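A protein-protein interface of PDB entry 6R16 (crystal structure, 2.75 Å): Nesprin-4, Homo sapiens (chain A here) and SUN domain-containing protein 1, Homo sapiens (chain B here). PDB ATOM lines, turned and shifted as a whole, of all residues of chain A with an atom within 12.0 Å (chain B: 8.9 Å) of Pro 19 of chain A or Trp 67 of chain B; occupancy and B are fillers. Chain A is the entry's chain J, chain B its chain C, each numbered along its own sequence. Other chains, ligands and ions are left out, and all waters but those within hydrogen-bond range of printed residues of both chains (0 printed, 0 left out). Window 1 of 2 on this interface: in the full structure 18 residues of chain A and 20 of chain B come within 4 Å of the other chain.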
ATOM      1  N   PRO A   8     -12.619   4.062  39.339  1.00  0.00           N
ATOM      2  CA  PRO A   8     -13.399   5.218  38.882  1.00  0.00           C
ATOM      3  C   PRO A   8     -14.604   5.463  39.775  1.00  0.00           C
ATOM      4  O   PRO A   8     -15.305   4.532  40.177  1.00  0.00           O
ATOM      5  CB  PRO A   8     -13.824   4.821  37.464  1.00  0.00           C
ATOM      6  CG  PRO A   8     -13.851   3.328  37.495  1.00  0.00           C
ATOM      7  CD  PRO A   8     -12.737   2.915  38.422  1.00  0.00           C
ATOM      8  N   CYS A   9     -14.841   6.738  40.083  1.00  0.00           N
ATOM      9  CA  CYS A   9     -15.962   7.129  40.929  1.00  0.00           C
ATOM     10  C   CYS A   9     -17.283   7.193  40.175  1.00  0.00           C
ATOM     11  O   CYS A   9     -18.308   7.519  40.784  1.00  0.00           O
ATOM     12  CB  CYS A   9     -15.679   8.484  41.584  1.00  0.00           C
ATOM     13  SG  CYS A   9     -14.277   8.481  42.723  1.00  0.00           S
ATOM     14  N   CYS A  10     -17.288   6.893  38.878  1.00  0.00           N
ATOM     15  CA  CYS A  10     -18.507   6.938  38.086  1.00  0.00           C
ATOM     16  C   CYS A  10     -18.293   6.125  36.819  1.00  0.00           C
ATOM     17  O   CYS A  10     -17.174   5.718  36.498  1.00  0.00           O
ATOM     18  CB  CYS A  10     -18.897   8.383  37.755  1.00  0.00           C
ATOM     19  SG  CYS A  10     -20.518   8.562  36.997  1.00  0.00           S
ATOM     20  N   SER A  11     -19.389   5.894  36.095  1.00  0.00           N
ATOM     21  CA  SER A  11     -19.341   5.155  34.844  1.00  0.00           C
ATOM     22  C   SER A  11     -19.593   6.020  33.618  1.00  0.00           C
ATOM     23  O   SER A  11     -19.404   5.541  32.495  1.00  0.00           O
ATOM     24  CB  SER A  11     -20.358   4.003  34.864  1.00  0.00           C
ATOM     25  OG  SER A  11     -19.967   2.992  35.778  1.00  0.00           O
ATOM     26  N   HIS A  12     -20.011   7.272  33.796  1.00  0.00           N
ATOM     27  CA  HIS A  12     -20.205   8.170  32.667  1.00  0.00           C
ATOM     28  C   HIS A  12     -18.864   8.746  32.235  1.00  0.00           C
ATOM     29  O   HIS A  12     -18.140   9.328  33.048  1.00  0.00           O
ATOM     30  CB  HIS A  12     -21.165   9.295  33.046  1.00  0.00           C
ATOM     31  CG  HIS A  12     -22.508   8.814  33.498  1.00  0.00           C
ATOM     32  ND1 HIS A  12     -22.909   8.867  34.816  1.00  0.00           N
ATOM     33  CD2 HIS A  12     -23.537   8.262  32.813  1.00  0.00           C
ATOM     34  CE1 HIS A  12     -24.130   8.373  34.922  1.00  0.00           C
ATOM     35  NE2 HIS A  12     -24.533   7.999  33.721  1.00  0.00           N
ATOM     36  N   ALA A  13     -18.539   8.598  30.954  1.00  0.00           N
ATOM     37  CA  ALA A  13     -17.277   9.118  30.447  1.00  0.00           C
ATOM     38  C   ALA A  13     -17.289  10.642  30.420  1.00  0.00           C
ATOM     39  O   ALA A  13     -18.308  11.267  30.116  1.00  0.00           O
ATOM     40  CB  ALA A  13     -17.001   8.570  29.047  1.00  0.00           C
ATOM     41  N   ARG A  14     -16.139  11.240  30.739  1.00  0.00           N
ATOM     42  CA  ARG A  14     -16.018  12.693  30.665  1.00  0.00           C
ATOM     43  C   ARG A  14     -15.975  13.169  29.218  1.00  0.00           C
ATOM     44  O   ARG A  14     -16.480  14.252  28.907  1.00  0.00           O
ATOM     45  CB  ARG A  14     -14.777  13.162  31.426  1.00  0.00           C
ATOM     46  CG  ARG A  14     -14.842  14.608  31.895  1.00  0.00           C
ATOM     47  CD  ARG A  14     -16.026  14.843  32.827  1.00  0.00           C
ATOM     48  NE  ARG A  14     -15.936  14.057  34.057  1.00  0.00           N
ATOM     49  CZ  ARG A  14     -15.433  14.507  35.202  1.00  0.00           C
ATOM     50  NH1 ARG A  14     -14.968  15.747  35.286  1.00  0.00           N
ATOM     51  NH2 ARG A  14     -15.395  13.718  36.267  1.00  0.00           N
ATOM     52  N   ILE A  15     -15.380  12.379  28.331  1.00  0.00           N
ATOM     53  CA  ILE A  15     -15.307  12.704  26.910  1.00  0.00           C
ATOM     54  C   ILE A  15     -16.479  12.016  26.218  1.00  0.00           C
ATOM     55  O   ILE A  15     -16.610  10.787  26.327  1.00  0.00           O
ATOM     56  CB  ILE A  15     -13.972  12.259  26.299  1.00  0.00           C
ATOM     57  CG1 ILE A  15     -12.797  12.862  27.074  1.00  0.00           C
ATOM     58  CG2 ILE A  15     -13.902  12.647  24.830  1.00  0.00           C
ATOM     59  CD1 ILE A  15     -12.712  14.367  26.975  1.00  0.00           C
ATOM     60  N   PRO A  16     -17.343  12.752  25.511  1.00  0.00           N
ATOM     61  CA  PRO A  16     -18.545  12.110  24.945  1.00  0.00           C
ATOM     62  C   PRO A  16     -18.237  11.058  23.892  1.00  0.00           C
ATOM     63  O   PRO A  16     -18.699   9.916  24.010  1.00  0.00           O
ATOM     64  CB  PRO A  16     -19.328  13.298  24.366  1.00  0.00           C
ATOM     65  CG  PRO A  16     -18.301  14.355  24.121  1.00  0.00           C
ATOM     66  CD  PRO A  16     -17.273  14.190  25.201  1.00  0.00           C
ATOM     67  N   ARG A  17     -17.467  11.405  22.866  1.00  0.00           N
ATOM     68  CA  ARG A  17     -17.152  10.483  21.784  1.00  0.00           C
ATOM     69  C   ARG A  17     -15.814   9.803  22.045  1.00  0.00           C
ATOM     70  O   ARG A  17     -14.871  10.429  22.538  1.00  0.00           O
ATOM     71  CB  ARG A  17     -17.125  11.208  20.437  1.00  0.00           C
ATOM     72  CG  ARG A  17     -16.255  12.454  20.405  1.00  0.00           C
ATOM     73  CD  ARG A  17     -16.316  13.127  19.043  1.00  0.00           C
ATOM     74  NE  ARG A  17     -15.881  12.231  17.974  1.00  0.00           N
ATOM     75  CZ  ARG A  17     -15.859  12.558  16.686  1.00  0.00           C
ATOM     76  NH1 ARG A  17     -16.248  13.765  16.297  1.00  0.00           N
ATOM     77  NH2 ARG A  17     -15.447  11.677  15.784  1.00  0.00           N
ATOM     78  N   THR A  18     -15.743   8.521  21.714  1.00  0.00           N
ATOM     79  CA  THR A  18     -14.529   7.743  21.940  1.00  0.00           C
ATOM     80  C   THR A  18     -13.436   8.185  20.975  1.00  0.00           C
ATOM     81  O   THR A  18     -13.649   8.149  19.756  1.00  0.00           O
ATOM     82  CB  THR A  18     -14.816   6.253  21.773  1.00  0.00           C
ATOM     83  OG1 THR A  18     -15.072   5.965  20.394  1.00  0.00           O
ATOM     84  CG2 THR A  18     -16.027   5.848  22.602  1.00  0.00           C
ATOM     85  N   PRO A  19     -12.275   8.616  21.460  1.00  0.00           N
ATOM     86  CA  PRO A  19     -11.226   9.092  20.554  1.00  0.00           C
ATOM     87  C   PRO A  19     -10.646   7.965  19.713  1.00  0.00           C
ATOM     88  O   PRO A  19     -10.769   6.779  20.029  1.00  0.00           O
ATOM     89  CB  PRO A  19     -10.171   9.671  21.504  1.00  0.00           C
ATOM     90  CG  PRO A  19     -10.386   8.942  22.788  1.00  0.00           C
ATOM     91  CD  PRO A  19     -11.864   8.681  22.874  1.00  0.00           C
ATOM     92  N   TYR A  20     -10.000   8.362  18.619  1.00  0.00           N
ATOM     93  CA  TYR A  20      -9.314   7.426  17.736  1.00  0.00           C
ATOM     94  C   TYR A  20      -8.097   8.126  17.151  1.00  0.00           C
ATOM     95  O   TYR A  20      -8.243   9.118  16.431  1.00  0.00           O
ATOM     96  CB  TYR A  20     -10.231   6.935  16.610  1.00  0.00           C
ATOM     97  CG  TYR A  20     -11.455   6.173  17.066  1.00  0.00           C
ATOM     98  CD1 TYR A  20     -11.357   4.858  17.504  1.00  0.00           C
ATOM     99  CD2 TYR A  20     -12.713   6.762  17.035  1.00  0.00           C
ATOM    100  CE1 TYR A  20     -12.476   4.155  17.914  1.00  0.00           C
ATOM    101  CE2 TYR A  20     -13.837   6.066  17.442  1.00  0.00           C
ATOM    102  CZ  TYR A  20     -13.713   4.765  17.880  1.00  0.00           C
ATOM    103  OH  TYR A  20     -14.831   4.072  18.286  1.00  0.00           O
ATOM    104  N   LEU A  21      -6.906   7.618  17.458  1.00  0.00           N
ATOM    105  CA  LEU A  21      -5.687   8.129  16.843  1.00  0.00           C
ATOM    106  C   LEU A  21      -5.592   7.608  15.416  1.00  0.00           C
ATOM    107  O   LEU A  21      -5.478   6.397  15.199  1.00  0.00           O
ATOM    108  CB  LEU A  21      -4.460   7.713  17.649  1.00  0.00           C
ATOM    109  CG  LEU A  21      -4.145   8.522  18.906  1.00  0.00           C
ATOM    110  CD1 LEU A  21      -2.913   7.961  19.598  1.00  0.00           C
ATOM    111  CD2 LEU A  21      -3.950   9.989  18.560  1.00  0.00           C
ATOM    112  N   VAL A  22      -5.649   8.514  14.445  1.00  0.00           N
ATOM    113  CA  VAL A  22      -5.597   8.161  13.031  1.00  0.00           C
ATOM    114  C   VAL A  22      -4.160   8.282  12.546  1.00  0.00           C
ATOM    115  O   VAL A  22      -3.484   9.280  12.823  1.00  0.00           O
ATOM    116  CB  VAL A  22      -6.534   9.053  12.197  1.00  0.00           C
ATOM    117  CG1 VAL A  22      -6.518   8.623  10.737  1.00  0.00           C
ATOM    118  CG2 VAL A  22      -7.947   9.001  12.755  1.00  0.00           C
ATOM    119  N   LEU A  23      -3.693   7.269  11.824  1.00  0.00           N
ATOM    120  CA  LEU A  23      -2.375   7.280  11.203  1.00  0.00           C
ATOM    121  C   LEU A  23      -2.567   7.298   9.692  1.00  0.00           C
ATOM    122  O   LEU A  23      -3.231   6.418   9.137  1.00  0.00           O
ATOM    123  CB  LEU A  23      -1.548   6.069  11.638  1.00  0.00           C
ATOM    124  CG  LEU A  23      -0.052   6.044  11.297  1.00  0.00           C
ATOM    125  CD1 LEU A  23       0.706   5.204  12.310  1.00  0.00           C
ATOM    126  CD2 LEU A  23       0.198   5.517   9.893  1.00  0.00           C
ATOM    127  N   THR B  51     -17.341   2.176  13.342  1.00  0.00           N
ATOM    128  CA  THR B  51     -16.896   1.219  14.344  1.00  0.00           C
ATOM    129  C   THR B  51     -18.020   0.924  15.328  1.00  0.00           C
ATOM    130  O   THR B  51     -18.694   1.840  15.809  1.00  0.00           O
ATOM    131  CB  THR B  51     -15.674   1.760  15.087  1.00  0.00           C
ATOM    132  OG1 THR B  51     -14.621   2.029  14.152  1.00  0.00           O
ATOM    133  CG2 THR B  51     -15.184   0.755  16.115  1.00  0.00           C
ATOM    134  N   GLU B  53     -19.705   0.625  18.519  1.00  0.00           N
ATOM    135  CA  GLU B  53     -19.469   1.219  19.829  1.00  0.00           C
ATOM    136  C   GLU B  53     -20.203   0.425  20.902  1.00  0.00           C
ATOM    137  O   GLU B  53     -21.416   0.217  20.804  1.00  0.00           O
ATOM    138  CB  GLU B  53     -19.893   2.688  19.860  1.00  0.00           C
ATOM    139  CG  GLU B  53     -19.140   3.557  18.864  1.00  0.00           C
ATOM    140  CD  GLU B  53     -19.638   4.987  18.835  1.00  0.00           C
ATOM    141  OE1 GLU B  53     -20.507   5.334  19.662  1.00  0.00           O
ATOM    142  OE2 GLU B  53     -19.151   5.767  17.990  1.00  0.00           O
ATOM    143  N   LYS B  55     -19.069   0.865  24.547  1.00  0.00           N
ATOM    144  CA  LYS B  55     -18.954   1.651  25.776  1.00  0.00           C
ATOM    145  C   LYS B  55     -18.896   0.741  27.004  1.00  0.00           C
ATOM    146  O   LYS B  55     -19.707   0.834  27.928  1.00  0.00           O
ATOM    147  CB  LYS B  55     -20.095   2.668  25.891  1.00  0.00           C
ATOM    148  CG  LYS B  55     -20.099   3.721  24.796  1.00  0.00           C
ATOM    149  CD  LYS B  55     -21.228   4.719  24.991  1.00  0.00           C
ATOM    150  CE  LYS B  55     -21.234   5.766  23.888  1.00  0.00           C
ATOM    151  NZ  LYS B  55     -19.946   6.513  23.821  1.00  0.00           N
ATOM    152  N   THR B  56     -17.910  -0.152  26.994  1.00  0.00           N
ATOM    153  CA  THR B  56     -17.664  -1.054  28.111  1.00  0.00           C
ATOM    154  C   THR B  56     -16.273  -0.905  28.706  1.00  0.00           C
ATOM    155  O   THR B  56     -16.117  -1.011  29.923  1.00  0.00           O
ATOM    156  CB  THR B  56     -17.888  -2.514  27.679  1.00  0.00           C
ATOM    157  OG1 THR B  56     -17.546  -3.393  28.758  1.00  0.00           O
ATOM    158  CG2 THR B  56     -17.052  -2.858  26.451  1.00  0.00           C
ATOM    159  N   ALA B  57     -15.256  -0.647  27.883  1.00  0.00           N
ATOM    160  CA  ALA B  57     -13.880  -0.518  28.360  1.00  0.00           C
ATOM    161  C   ALA B  57     -13.663   0.926  28.792  1.00  0.00           C
ATOM    162  O   ALA B  57     -13.236   1.777  28.012  1.00  0.00           O
ATOM    163  CB  ALA B  57     -12.892  -0.940  27.279  1.00  0.00           C
ATOM    164  N   LEU B  58     -13.953   1.203  30.061  1.00  0.00           N
ATOM    165  CA  LEU B  58     -13.874   2.555  30.600  1.00  0.00           C
ATOM    166  C   LEU B  58     -12.455   2.843  31.072  1.00  0.00           C
ATOM    167  O   LEU B  58     -11.959   2.194  31.999  1.00  0.00           O
ATOM    168  CB  LEU B  58     -14.866   2.736  31.749  1.00  0.00           C
ATOM    169  CG  LEU B  58     -14.875   4.115  32.416  1.00  0.00           C
ATOM    170  CD1 LEU B  58     -15.155   5.207  31.397  1.00  0.00           C
ATOM    171  CD2 LEU B  58     -15.891   4.163  33.547  1.00  0.00           C
ATOM    172  N   MET B  59     -11.806   3.812  30.433  1.00  0.00           N
ATOM    173  CA  MET B  59     -10.483   4.263  30.845  1.00  0.00           C
ATOM    174  C   MET B  59     -10.632   5.424  31.819  1.00  0.00           C
ATOM    175  O   MET B  59     -11.309   6.412  31.518  1.00  0.00           O
ATOM    176  CB  MET B  59      -9.652   4.689  29.634  1.00  0.00           C
ATOM    177  CG  MET B  59      -9.517   3.622  28.557  1.00  0.00           C
ATOM    178  SD  MET B  59      -8.670   2.143  29.144  1.00  0.00           S
ATOM    179  CE  MET B  59      -7.092   2.828  29.647  1.00  0.00           C
ATOM    180  N   SER B  60     -10.000   5.304  32.983  1.00  0.00           N
ATOM    181  CA  SER B  60     -10.092   6.315  34.024  1.00  0.00           C
ATOM    182  C   SER B  60      -8.702   6.648  34.548  1.00  0.00           C
ATOM    183  O   SER B  60      -7.753   5.873  34.398  1.00  0.00           O
ATOM    184  CB  SER B  60     -10.997   5.857  35.176  1.00  0.00           C
ATOM    185  OG  SER B  60     -10.533   4.643  35.738  1.00  0.00           O
ATOM    186  N   LEU B  61      -8.596   7.824  35.162  1.00  0.00           N
ATOM    187  CA  LEU B  61      -7.342   8.299  35.728  1.00  0.00           C
ATOM    188  C   LEU B  61      -7.650   9.110  36.979  1.00  0.00           C
ATOM    189  O   LEU B  61      -8.440  10.057  36.921  1.00  0.00           O
ATOM    190  CB  LEU B  61      -6.562   9.142  34.713  1.00  0.00           C
ATOM    191  CG  LEU B  61      -5.196   9.672  35.149  1.00  0.00           C
ATOM    192  CD1 LEU B  61      -4.268   8.528  35.525  1.00  0.00           C
ATOM    193  CD2 LEU B  61      -4.583  10.524  34.050  1.00  0.00           C
ATOM    194  N   ILE B  64     -11.224   9.523  37.852  1.00  0.00           N
ATOM    195  CA  ILE B  64     -12.034  10.332  36.947  1.00  0.00           C
ATOM    196  C   ILE B  64     -12.224   9.535  35.661  1.00  0.00           C
ATOM    197  O   ILE B  64     -11.237   9.292  34.945  1.00  0.00           O
ATOM    198  CB  ILE B  64     -11.383  11.691  36.667  1.00  0.00           C
ATOM    199  CG1 ILE B  64     -11.154  12.454  37.973  1.00  0.00           C
ATOM    200  CG2 ILE B  64     -12.240  12.506  35.711  1.00  0.00           C
ATOM    201  CD1 ILE B  64     -10.468  13.788  37.785  1.00  0.00           C
ATOM    202  N   PRO B  65     -13.443   9.110  35.326  1.00  0.00           N
ATOM    203  CA  PRO B  65     -13.657   8.412  34.052  1.00  0.00           C
ATOM    204  C   PRO B  65     -13.397   9.349  32.882  1.00  0.00           C
ATOM    205  O   PRO B  65     -13.952  10.448  32.815  1.00  0.00           O
ATOM    206  CB  PRO B  65     -15.126   7.980  34.122  1.00  0.00           C
ATOM    207  CG  PRO B  65     -15.751   8.944  35.084  1.00  0.00           C
ATOM    208  CD  PRO B  65     -14.691   9.261  36.095  1.00  0.00           C
ATOM    209  N   LEU B  66     -12.553   8.903  31.952  1.00  0.00           N
ATOM    210  CA  LEU B  66     -12.111   9.743  30.843  1.00  0.00           C
ATOM    211  C   LEU B  66     -12.819   9.401  29.536  1.00  0.00           C
ATOM    212  O   LEU B  66     -13.452  10.270  28.930  1.00  0.00           O
ATOM    213  CB  LEU B  66     -10.590   9.634  30.684  1.00  0.00           C
ATOM    214  CG  LEU B  66      -9.762  10.078  31.891  1.00  0.00           C
ATOM    215  CD1 LEU B  66      -8.276  10.018  31.578  1.00  0.00           C
ATOM    216  CD2 LEU B  66     -10.161  11.479  32.329  1.00  0.00           C
ATOM    217  N   TRP B  67     -12.743   8.146  29.098  1.00  0.00           N
ATOM    218  CA  TRP B  67     -13.361   7.760  27.836  1.00  0.00           C
ATOM    219  C   TRP B  67     -13.461   6.244  27.769  1.00  0.00           C
ATOM    220  O   TRP B  67     -12.787   5.523  28.509  1.00  0.00           O
ATOM    221  CB  TRP B  67     -12.565   8.284  26.633  1.00  0.00           C
ATOM    222  CG  TRP B  67     -11.143   7.795  26.588  1.00  0.00           C
ATOM    223  CD1 TRP B  67     -10.714   6.553  26.212  1.00  0.00           C
ATOM    224  CD2 TRP B  67      -9.965   8.537  26.930  1.00  0.00           C
ATOM    225  NE1 TRP B  67      -9.345   6.476  26.300  1.00  0.00           N
ATOM    226  CE2 TRP B  67      -8.862   7.680  26.739  1.00  0.00           C
ATOM    227  CE3 TRP B  67      -9.736   9.841  27.378  1.00  0.00           C
ATOM    228  CZ2 TRP B  67      -7.551   8.086  26.982  1.00  0.00           C
ATOM    229  CZ3 TRP B  67      -8.434  10.241  27.621  1.00  0.00           C
ATOM    230  CH2 TRP B  67      -7.358   9.367  27.421  1.00  0.00           C
ATOM    231  N   TYR B  68     -14.318   5.774  26.867  1.00  0.00           N
ATOM    232  CA  TYR B  68     -14.436   4.355  26.570  1.00  0.00           C
ATOM    233  C   TYR B  68     -13.504   3.978  25.426  1.00  0.00           C
ATOM    234  O   TYR B  68     -13.414   4.691  24.422  1.00  0.00           O
ATOM    235  CB  TYR B  68     -15.880   3.994  26.220  1.00  0.00           C
ATOM    236  CG  TYR B  68     -16.817   4.058  27.403  1.00  0.00           C
ATOM    237  CD1 TYR B  68     -16.851   3.033  28.339  1.00  0.00           C
ATOM    238  CD2 TYR B  68     -17.658   5.147  27.592  1.00  0.00           C
ATOM    239  CE1 TYR B  68     -17.704   3.085  29.427  1.00  0.00           C
ATOM    240  CE2 TYR B  68     -18.515   5.209  28.679  1.00  0.00           C
ATOM    241  CZ  TYR B  68     -18.531   4.173  29.593  1.00  0.00           C
ATOM    242  OH  TYR B  68     -19.378   4.224  30.676  1.00  0.00           O
ATOM    243  N   PHE B  69     -12.808   2.856  25.584  1.00  0.00           N
ATOM    244  CA  PHE B  69     -11.840   2.404  24.592  1.00  0.00           C
ATOM    245  C   PHE B  69     -12.476   1.410  23.628  1.00  0.00           C
ATOM    246  O   PHE B  69     -13.150   0.466  24.052  1.00  0.00           O
ATOM    247  CB  PHE B  69     -10.624   1.767  25.265  1.00  0.00           C
ATOM    248  CG  PHE B  69      -9.686   1.108  24.299  1.00  0.00           C
ATOM    249  CD1 PHE B  69      -8.849   1.868  23.499  1.00  0.00           C
ATOM    250  CD2 PHE B  69      -9.639  -0.272  24.186  1.00  0.00           C
ATOM    251  CE1 PHE B  69      -7.987   1.267  22.604  1.00  0.00           C
ATOM    252  CE2 PHE B  69      -8.778  -0.880  23.294  1.00  0.00           C
ATOM    253  CZ  PHE B  69      -7.951  -0.109  22.502  1.00  0.00           C
ATOM    254  N   SER B  70     -12.240   1.620  22.334  1.00  0.00           N
ATOM    255  CA  SER B  70     -12.674   0.702  21.292  1.00  0.00           C
ATOM    256  C   SER B  70     -11.607   0.651  20.210  1.00  0.00           C
ATOM    257  O   SER B  70     -11.014   1.678  19.866  1.00  0.00           O
ATOM    258  CB  SER B  70     -14.016   1.129  20.684  1.00  0.00           C
ATOM    259  OG  SER B  70     -15.060   1.035  21.635  1.00  0.00           O
ATOM    260  N   GLN B  71     -11.365  -0.544  19.679  1.00  0.00           N
ATOM    261  CA  GLN B  71     -10.329  -0.713  18.670  1.00  0.00           C
ATOM    262  C   GLN B  71     -10.751  -0.068  17.355  1.00  0.00           C
ATOM    263  O   GLN B  71     -11.886  -0.242  16.898  1.00  0.00           O
ATOM    264  CB  GLN B  71     -10.031  -2.198  18.455  1.00  0.00           C
ATOM    265  CG  GLN B  71      -9.579  -2.947  19.703  1.00  0.00           C
ATOM    266  CD  GLN B  71      -8.144  -2.646  20.100  1.00  0.00           C
ATOM    267  OE1 GLN B  71      -7.474  -1.817  19.487  1.00  0.00           O
ATOM    268  NE2 GLN B  71      -7.665  -3.328  21.136  1.00  0.00           N
ATOM    269  N   SER B  72      -9.836   0.670  16.747  1.00  0.00           N
ATOM    270  CA  SER B  72     -10.059   1.304  15.456  1.00  0.00           C
ATOM    271  C   SER B  72      -9.747   0.321  14.339  1.00  0.00           C
ATOM    272  O   SER B  72      -9.192  -0.755  14.575  1.00  0.00           O
ATOM    273  CB  SER B  72      -9.195   2.557  15.347  1.00  0.00           C
ATOM    274  OG  SER B  72      -7.818   2.225  15.298  1.00  0.00           O
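The backbone carbonyl oxygen (O) of Met 59 of chain B is in hydrogen-bond range of the backbone NH (N) of Leu 66 of chain B (2.8 Å).
The side-chain hydroxyl (OG1) of Thr 18 of chain A sits at hydrogen-bond distance from the side-chain hydroxyl (OH) of Tyr 20 of chain A (2.8 Å).
The backbone NH of Met 59 of chain B is in hydrogen-bond range of the backbone carbonyl oxygen of Trp 67 of chain B (2.8 Å).
Hydrophobic or aromatic side chains of chain A within 4 Å of the printed part of chain B: Pro 8, Ala 13, Ile 15, Pro 19 and Tyr 20.
The backbone carbonyl oxygen of Ser 11 of chain A sits close to the side-chain hydroxyl of Tyr 68 of chain B (2.2 Å).
The backbone NH of Arg 14 of chain A is in hydrogen-bond range of the backbone carbonyl oxygen of Pro 65 of chain B (3.1 Å).
The backbone NH of Arg 14 of chain A sits at hydrogen-bond distance from the backbone carbonyl oxygen of Leu 66 of chain B, at 3.4 Å.
The backbone carbonyl oxygen (O) of Leu 66 of chain B lies within hydrogen-bond range of the backbone NH (N) of Ile 15 of chain A, at 2.9 Å.
CB of Pro 8 of chain A touches OG of Ser 60 of chain B (3.7 Å).
O of Cys 10 of chain A touches CD2 of Leu 58 of chain B, at 3.6 Å.
Pro 65 of chain B touches His 12 of chain A.
CB of Ala 13 of chain A touches O of Leu 66 of chain B, at 3.9 Å.
Ala 13 of chain A touches Trp 67 of chain B.
Ala 13 of chain A touches Tyr 68 of chain B (CB to CE2, 3.7 Å).
Arg 14 of chain A touches Ile 64 of chain B (NH2 to CG2, 3.4 Å).
Thr 51 of chain B touches Tyr 20 of chain A.
Tyr 20 of chain A touches Ser 70 of chain B.
CD1 of Tyr 20 of chain A touches CB of Ser 72 of chain B, 3.8 Å away.
Trp 67 of chain B touches just these residues of chain A: Ala 13 (3.9 Å) and Pro 19 (3.8 Å).
No residue of chain A comes within 4 Å of Ala 57 of chain B.
No residue of chain A comes within 4 Å of Met 59 of chain B.
Ser 60 of chain B touches one residue of chain A.
Pro 65 of chain B touches three residues of chain A.
Tyr 68 of chain B touches just these residues of chain A: Ser 11 (2.2 Å), Ala 13 (3.7 Å) and Thr 18 (3.4 Å).
Ser 70 of chain B touches just one residue of chain A: Tyr 20 (3.5 Å).
Of the printed residues of chain B, Pro 16 of chain A touches Lys 55.
Of the printed residues of chain A, Ser 72 of chain B touches Tyr 20.
Printed residues of chain A within 4 Å of Thr 51 of chain B: Tyr 20 (3.98 Å).
Val 22 of chain A touches none of the printed residues of chain B.
Leu 21 of chain A touches none of the printed residues of chain B.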
